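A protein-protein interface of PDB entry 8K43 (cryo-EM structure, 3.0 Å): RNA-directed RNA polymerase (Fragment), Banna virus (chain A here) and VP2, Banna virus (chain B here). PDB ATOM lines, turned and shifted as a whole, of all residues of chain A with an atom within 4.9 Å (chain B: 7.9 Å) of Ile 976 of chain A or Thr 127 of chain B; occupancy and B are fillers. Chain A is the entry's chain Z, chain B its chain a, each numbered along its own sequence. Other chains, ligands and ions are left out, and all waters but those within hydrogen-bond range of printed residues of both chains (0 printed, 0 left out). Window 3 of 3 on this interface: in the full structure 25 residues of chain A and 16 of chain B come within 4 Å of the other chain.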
ATOM      1  N   ASP A 972      22.278 -40.399  -3.099  1.00  0.00           N
ATOM      2  CA  ASP A 972      22.268 -39.506  -1.950  1.00  0.00           C
ATOM      3  C   ASP A 972      23.591 -38.772  -1.788  1.00  0.00           C
ATOM      4  O   ASP A 972      23.627 -37.700  -1.176  1.00  0.00           O
ATOM      5  CB  ASP A 972      21.928 -40.306  -0.687  1.00  0.00           C
ATOM      6  CG  ASP A 972      20.480 -40.759  -0.642  1.00  0.00           C
ATOM      7  OD1 ASP A 972      19.659 -40.233  -1.424  1.00  0.00           O
ATOM      8  OD2 ASP A 972      20.159 -41.645   0.179  1.00  0.00           O
ATOM      9  N   GLY A 974      27.249 -37.943  -0.286  1.00  0.00           N
ATOM     10  CA  GLY A 974      27.785 -38.026   1.056  1.00  0.00           C
ATOM     11  C   GLY A 974      26.845 -37.399   2.060  1.00  0.00           C
ATOM     12  O   GLY A 974      27.254 -37.029   3.164  1.00  0.00           O
ATOM     13  N   GLY A 975      25.576 -37.278   1.683  1.00  0.00           N
ATOM     14  CA  GLY A 975      24.621 -36.532   2.472  1.00  0.00           C
ATOM     15  C   GLY A 975      24.650 -35.043   2.232  1.00  0.00           C
ATOM     16  O   GLY A 975      23.991 -34.299   2.966  1.00  0.00           O
ATOM     17  N   ILE A 976      25.391 -34.584   1.225  1.00  0.00           N
ATOM     18  CA  ILE A 976      25.556 -33.161   0.959  1.00  0.00           C
ATOM     19  C   ILE A 976      24.259 -32.584   0.416  1.00  0.00           C
ATOM     20  O   ILE A 976      23.344 -33.323   0.039  1.00  0.00           O
ATOM     21  CB  ILE A 976      26.723 -32.908  -0.011  1.00  0.00           C
ATOM     22  CG1 ILE A 976      26.507 -33.664  -1.318  1.00  0.00           C
ATOM     23  CG2 ILE A 976      28.037 -33.321   0.622  1.00  0.00           C
ATOM     24  CD1 ILE A 976      27.111 -32.977  -2.516  1.00  0.00           C
ATOM     25  N   HIS A 977      24.173 -31.259   0.374  1.00  0.00           N
ATOM     26  CA  HIS A 977      22.972 -30.574  -0.085  1.00  0.00           C
ATOM     27  C   HIS A 977      22.913 -30.645  -1.604  1.00  0.00           C
ATOM     28  O   HIS A 977      23.756 -30.062  -2.293  1.00  0.00           O
ATOM     29  CB  HIS A 977      22.972 -29.128   0.400  1.00  0.00           C
ATOM     30  CG  HIS A 977      22.066 -28.230  -0.378  1.00  0.00           C
ATOM     31  ND1 HIS A 977      20.708 -28.169  -0.156  1.00  0.00           N
ATOM     32  CD2 HIS A 977      22.323 -27.354  -1.377  1.00  0.00           C
ATOM     33  CE1 HIS A 977      20.166 -27.293  -0.983  1.00  0.00           C
ATOM     34  NE2 HIS A 977      21.126 -26.784  -1.736  1.00  0.00           N
ATOM     35  N   ILE A 978      21.921 -31.357  -2.128  1.00  0.00           N
ATOM     36  CA  ILE A 978      21.730 -31.492  -3.567  1.00  0.00           C
ATOM     37  C   ILE A 978      20.881 -30.319  -4.033  1.00  0.00           C
ATOM     38  O   ILE A 978      19.687 -30.247  -3.736  1.00  0.00           O
ATOM     39  CB  ILE A 978      21.076 -32.831  -3.923  1.00  0.00           C
ATOM     40  CG1 ILE A 978      21.698 -33.961  -3.105  1.00  0.00           C
ATOM     41  CG2 ILE A 978      21.211 -33.107  -5.409  1.00  0.00           C
ATOM     42  CD1 ILE A 978      23.079 -34.349  -3.559  1.00  0.00           C
ATOM     43  N   TYR A1107      28.466 -24.880  -6.373  1.00  0.00           N
ATOM     44  CA  TYR A1107      29.050 -25.549  -5.223  1.00  0.00           C
ATOM     45  C   TYR A1107      30.456 -25.035  -4.925  1.00  0.00           C
ATOM     46  O   TYR A1107      31.134 -24.505  -5.807  1.00  0.00           O
ATOM     47  CB  TYR A1107      29.100 -27.051  -5.468  1.00  0.00           C
ATOM     48  CG  TYR A1107      27.774 -27.747  -5.318  1.00  0.00           C
ATOM     49  CD1 TYR A1107      27.082 -27.709  -4.121  1.00  0.00           C
ATOM     50  CD2 TYR A1107      27.217 -28.447  -6.372  1.00  0.00           C
ATOM     51  CE1 TYR A1107      25.872 -28.348  -3.978  1.00  0.00           C
ATOM     52  CE2 TYR A1107      26.010 -29.087  -6.241  1.00  0.00           C
ATOM     53  CZ  TYR A1107      25.341 -29.037  -5.043  1.00  0.00           C
ATOM     54  OH  TYR A1107      24.132 -29.676  -4.911  1.00  0.00           O
ATOM     55  N   PRO A1108      30.917 -25.178  -3.682  1.00  0.00           N
ATOM     56  CA  PRO A1108      32.326 -24.905  -3.386  1.00  0.00           C
ATOM     57  C   PRO A1108      33.221 -25.925  -4.065  1.00  0.00           C
ATOM     58  O   PRO A1108      32.813 -27.059  -4.332  1.00  0.00           O
ATOM     59  CB  PRO A1108      32.401 -25.028  -1.862  1.00  0.00           C
ATOM     60  CG  PRO A1108      31.283 -25.936  -1.515  1.00  0.00           C
ATOM     61  CD  PRO A1108      30.184 -25.610  -2.481  1.00  0.00           C
ATOM     62  N   ASN A1111      34.048 -29.685  -2.673  1.00  0.00           N
ATOM     63  CA  ASN A1111      33.166 -30.807  -2.953  1.00  0.00           C
ATOM     64  C   ASN A1111      33.002 -31.088  -4.438  1.00  0.00           C
ATOM     65  O   ASN A1111      32.222 -31.977  -4.799  1.00  0.00           O
ATOM     66  CB  ASN A1111      31.790 -30.567  -2.328  1.00  0.00           C
ATOM     67  CG  ASN A1111      31.796 -30.753  -0.832  1.00  0.00           C
ATOM     68  OD1 ASN A1111      32.218 -29.872  -0.087  1.00  0.00           O
ATOM     69  ND2 ASN A1111      31.332 -31.911  -0.383  1.00  0.00           N
ATOM     70  N   THR A1114      32.848 -34.727  -5.640  1.00  0.00           N
ATOM     71  CA  THR A1114      31.595 -35.409  -5.334  1.00  0.00           C
ATOM     72  C   THR A1114      30.524 -35.042  -6.350  1.00  0.00           C
ATOM     73  O   THR A1114      29.767 -35.908  -6.811  1.00  0.00           O
ATOM     74  CB  THR A1114      31.138 -35.064  -3.918  1.00  0.00           C
ATOM     75  OG1 THR A1114      32.080 -35.586  -2.972  1.00  0.00           O
ATOM     76  CG2 THR A1114      29.775 -35.666  -3.633  1.00  0.00           C
ATOM     77  N   LEU A1118      28.084 -37.427  -8.911  1.00  0.00           N
ATOM     78  CA  LEU A1118      26.632 -37.478  -8.991  1.00  0.00           C
ATOM     79  C   LEU A1118      26.113 -37.206 -10.394  1.00  0.00           C
ATOM     80  O   LEU A1118      24.969 -37.557 -10.695  1.00  0.00           O
ATOM     81  CB  LEU A1118      26.020 -36.481  -8.008  1.00  0.00           C
ATOM     82  CG  LEU A1118      26.276 -36.794  -6.536  1.00  0.00           C
ATOM     83  CD1 LEU A1118      25.736 -35.692  -5.653  1.00  0.00           C
ATOM     84  CD2 LEU A1118      25.653 -38.127  -6.165  1.00  0.00           C
ATOM     85  N   ASP B 122      32.951 -19.513   1.526  1.00  0.00           N
ATOM     86  CA  ASP B 122      31.577 -19.287   1.101  1.00  0.00           C
ATOM     87  C   ASP B 122      30.930 -20.600   0.676  1.00  0.00           C
ATOM     88  O   ASP B 122      31.531 -21.390  -0.057  1.00  0.00           O
ATOM     89  CB  ASP B 122      31.534 -18.281  -0.047  1.00  0.00           C
ATOM     90  CG  ASP B 122      31.688 -16.850   0.428  1.00  0.00           C
ATOM     91  OD1 ASP B 122      31.873 -16.643   1.645  1.00  0.00           O
ATOM     92  OD2 ASP B 122      31.625 -15.931  -0.416  1.00  0.00           O
ATOM     93  N   LYS B 123      29.710 -20.836   1.164  1.00  0.00           N
ATOM     94  CA  LYS B 123      28.901 -21.999   0.809  1.00  0.00           C
ATOM     95  C   LYS B 123      29.519 -23.318   1.261  1.00  0.00           C
ATOM     96  O   LYS B 123      28.988 -24.389   0.954  1.00  0.00           O
ATOM     97  CB  LYS B 123      28.651 -22.037  -0.701  1.00  0.00           C
ATOM     98  CG  LYS B 123      27.652 -21.008  -1.196  1.00  0.00           C
ATOM     99  CD  LYS B 123      27.153 -21.353  -2.589  1.00  0.00           C
ATOM    100  CE  LYS B 123      27.483 -20.251  -3.583  1.00  0.00           C
ATOM    101  NZ  LYS B 123      26.484 -19.148  -3.547  1.00  0.00           N
ATOM    102  N   LEU B 124      30.636 -23.261   1.988  1.00  0.00           N
ATOM    103  CA  LEU B 124      31.304 -24.490   2.405  1.00  0.00           C
ATOM    104  C   LEU B 124      30.528 -25.179   3.521  1.00  0.00           C
ATOM    105  O   LEU B 124      30.297 -26.392   3.472  1.00  0.00           O
ATOM    106  CB  LEU B 124      32.738 -24.172   2.841  1.00  0.00           C
ATOM    107  CG  LEU B 124      33.855 -25.227   2.883  1.00  0.00           C
ATOM    108  CD1 LEU B 124      35.109 -24.616   3.490  1.00  0.00           C
ATOM    109  CD2 LEU B 124      33.485 -26.503   3.623  1.00  0.00           C
ATOM    110  N   TYR B 125      30.100 -24.420   4.528  1.00  0.00           N
ATOM    111  CA  TYR B 125      29.442 -25.028   5.679  1.00  0.00           C
ATOM    112  C   TYR B 125      28.055 -25.547   5.323  1.00  0.00           C
ATOM    113  O   TYR B 125      27.649 -26.619   5.787  1.00  0.00           O
ATOM    114  CB  TYR B 125      29.354 -24.023   6.824  1.00  0.00           C
ATOM    115  CG  TYR B 125      28.802 -24.603   8.102  1.00  0.00           C
ATOM    116  CD1 TYR B 125      29.521 -25.539   8.829  1.00  0.00           C
ATOM    117  CD2 TYR B 125      27.561 -24.214   8.586  1.00  0.00           C
ATOM    118  CE1 TYR B 125      29.023 -26.070   9.999  1.00  0.00           C
ATOM    119  CE2 TYR B 125      27.056 -24.741   9.756  1.00  0.00           C
ATOM    120  CZ  TYR B 125      27.792 -25.667  10.457  1.00  0.00           C
ATOM    121  OH  TYR B 125      27.293 -26.198  11.623  1.00  0.00           O
ATOM    122  N   ALA B 126      27.313 -24.804   4.503  1.00  0.00           N
ATOM    123  CA  ALA B 126      25.935 -25.182   4.212  1.00  0.00           C
ATOM    124  C   ALA B 126      25.855 -26.426   3.339  1.00  0.00           C
ATOM    125  O   ALA B 126      24.879 -27.179   3.429  1.00  0.00           O
ATOM    126  CB  ALA B 126      25.203 -24.022   3.541  1.00  0.00           C
ATOM    127  N   THR B 127      26.857 -26.659   2.492  1.00  0.00           N
ATOM    128  CA  THR B 127      26.779 -27.758   1.535  1.00  0.00           C
ATOM    129  C   THR B 127      26.953 -29.117   2.201  1.00  0.00           C
ATOM    130  O   THR B 127      26.324 -30.095   1.780  1.00  0.00           O
ATOM    131  CB  THR B 127      27.825 -27.574   0.438  1.00  0.00           C
ATOM    132  OG1 THR B 127      27.757 -26.236  -0.068  1.00  0.00           O
ATOM    133  CG2 THR B 127      27.584 -28.554  -0.700  1.00  0.00           C
ATOM    134  N   GLN B 128      27.787 -29.206   3.234  1.00  0.00           N
ATOM    135  CA  GLN B 128      28.085 -30.492   3.847  1.00  0.00           C
ATOM    136  C   GLN B 128      26.889 -31.036   4.625  1.00  0.00           C
ATOM    137  O   GLN B 128      25.942 -30.320   4.956  1.00  0.00           O
ATOM    138  CB  GLN B 128      29.303 -30.388   4.770  1.00  0.00           C
ATOM    139  CG  GLN B 128      30.524 -29.574   4.283  1.00  0.00           C
ATOM    140  CD  GLN B 128      30.749 -29.543   2.771  1.00  0.00           C
ATOM    141  OE1 GLN B 128      31.268 -28.565   2.240  1.00  0.00           O
ATOM    142  NE2 GLN B 128      30.460 -30.647   2.094  1.00  0.00           N
ATOM    143  N   SER B 129      26.956 -32.334   4.916  1.00  0.00           N
ATOM    144  CA  SER B 129      25.899 -33.030   5.627  1.00  0.00           C
ATOM    145  C   SER B 129      25.900 -32.643   7.104  1.00  0.00           C
ATOM    146  O   SER B 129      26.808 -31.975   7.603  1.00  0.00           O
ATOM    147  CB  SER B 129      26.059 -34.540   5.479  1.00  0.00           C
ATOM    148  OG  SER B 129      27.338 -34.957   5.919  1.00  0.00           O
ATOM    149  N   SER B 130      24.853 -33.079   7.807  1.00  0.00           N
ATOM    150  CA  SER B 130      24.687 -32.704   9.206  1.00  0.00           C
ATOM    151  C   SER B 130      25.824 -33.242  10.069  1.00  0.00           C
ATOM    152  O   SER B 130      26.362 -32.522  10.919  1.00  0.00           O
ATOM    153  CB  SER B 130      23.341 -33.208   9.722  1.00  0.00           C
ATOM    154  OG  SER B 130      22.279 -32.727   8.919  1.00  0.00           O
ATOM    155  N   ILE B 132      28.928 -34.051   9.188  1.00  0.00           N
ATOM    156  CA  ILE B 132      30.138 -33.287   8.913  1.00  0.00           C
ATOM    157  C   ILE B 132      29.998 -31.864   9.433  1.00  0.00           C
ATOM    158  O   ILE B 132      30.968 -31.267   9.912  1.00  0.00           O
ATOM    159  CB  ILE B 132      30.461 -33.318   7.409  1.00  0.00           C
ATOM    160  CG1 ILE B 132      30.534 -34.763   6.918  1.00  0.00           C
ATOM    161  CG2 ILE B 132      31.764 -32.594   7.127  1.00  0.00           C
ATOM    162  CD1 ILE B 132      31.798 -35.481   7.332  1.00  0.00           C
ATOM    163  N   GLN B 133      28.791 -31.300   9.353  1.00  0.00           N
ATOM    164  CA  GLN B 133      28.562 -29.968   9.904  1.00  0.00           C
ATOM    165  C   GLN B 133      28.822 -29.931  11.400  1.00  0.00           C
ATOM    166  O   GLN B 133      29.208 -28.887  11.937  1.00  0.00           O
ATOM    167  CB  GLN B 133      27.136 -29.509   9.607  1.00  0.00           C
ATOM    168  CG  GLN B 133      26.967 -28.822   8.267  1.00  0.00           C
ATOM    169  CD  GLN B 133      25.583 -28.238   8.090  1.00  0.00           C
ATOM    170  OE1 GLN B 133      24.905 -27.916   9.063  1.00  0.00           O
ATOM    171  NE2 GLN B 133      25.155 -28.098   6.841  1.00  0.00           N
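Of the 11 printed residues of chain A, 7 touch a printed residue of chain B. Hydrophobic or aromatic side chains of chain A that line the printed part of chain B: Ile 976, His 977, Tyr 1107 and Pro 1108. Among the printed residues, 9 pairs touch across the chains. Among the printed residues, no Asp or Glu carboxylate lies within 4 Å of a Lys or Arg side-chain nitrogen of the other chain.
O of Gly 974 of chain A sits at hydrogen-bond distance from OG of Ser 129 of chain B, 3.4 Å away. The backbone NH of His 977 of chain A is in hydrogen-bond range of the backbone carbonyl oxygen of Thr 127 of chain B (2.8 Å). The side-chain amide oxygen (OE1) of Gln 128 of chain B sits close to the side-chain amide oxygen (OD1) of Asn 1111 of chain A (2.8 Å).
O of Gly 975 of chain A touches CB of Ser 129 of chain B (3.3 Å). CA of Ile 976 of chain A touches O of Thr 127 of chain B, at 3.3 Å. Gln 128 of chain B touches Ile 976 of chain A (NE2 to CG2, 3.9 Å). CD1 of Tyr 1107 of chain A touches CG2 of Thr 127 of chain B, at 3.6 Å. CG of Pro 1108 of chain A touches O of Lys 123 of chain B, 3.7 Å away. Thr 127 of chain B touches Pro 1108 of chain A (OG1 to CD, 3.5 Å).
Ile 976 of chain A touches two residues of chain B. Of the printed residues of chain B, Tyr 1107 of chain A touches Thr 127. Printed residues of chain A within 4 Å of Gln 128 of chain B: Ile 976 (3.9 Å) and Asn 1111 (2.8 Å). Printed residues of chain A within 4 Å of Ser 129 of chain B: Gly 974 (3.4 Å) and Gly 975 (3.3 Å). The nearest printed residue of chain A that does not touch Ser 129 of chain B is Ile 976 of chain A (4.3 Å).
The backbone carbonyl oxygen (O) of His 977 of chain A sits at hydrogen-bond distance from the side-chain hydroxyl (OH) of Tyr 1107 of chain A, at 2.7 Å. The side-chain hydroxyl of Thr 127 of chain B lies within hydrogen-bond range of the backbone carbonyl oxygen of Lys 123 of chain B (2.4 Å). O of Leu 124 of chain B sits close to OE1 of Gln 128 of chain B, 2.7 Å away. The backbone carbonyl oxygen of Gln 128 of chain B sits at hydrogen-bond distance from the side-chain amide nitrogen of Gln 133 of chain B, 3.0 Å away.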
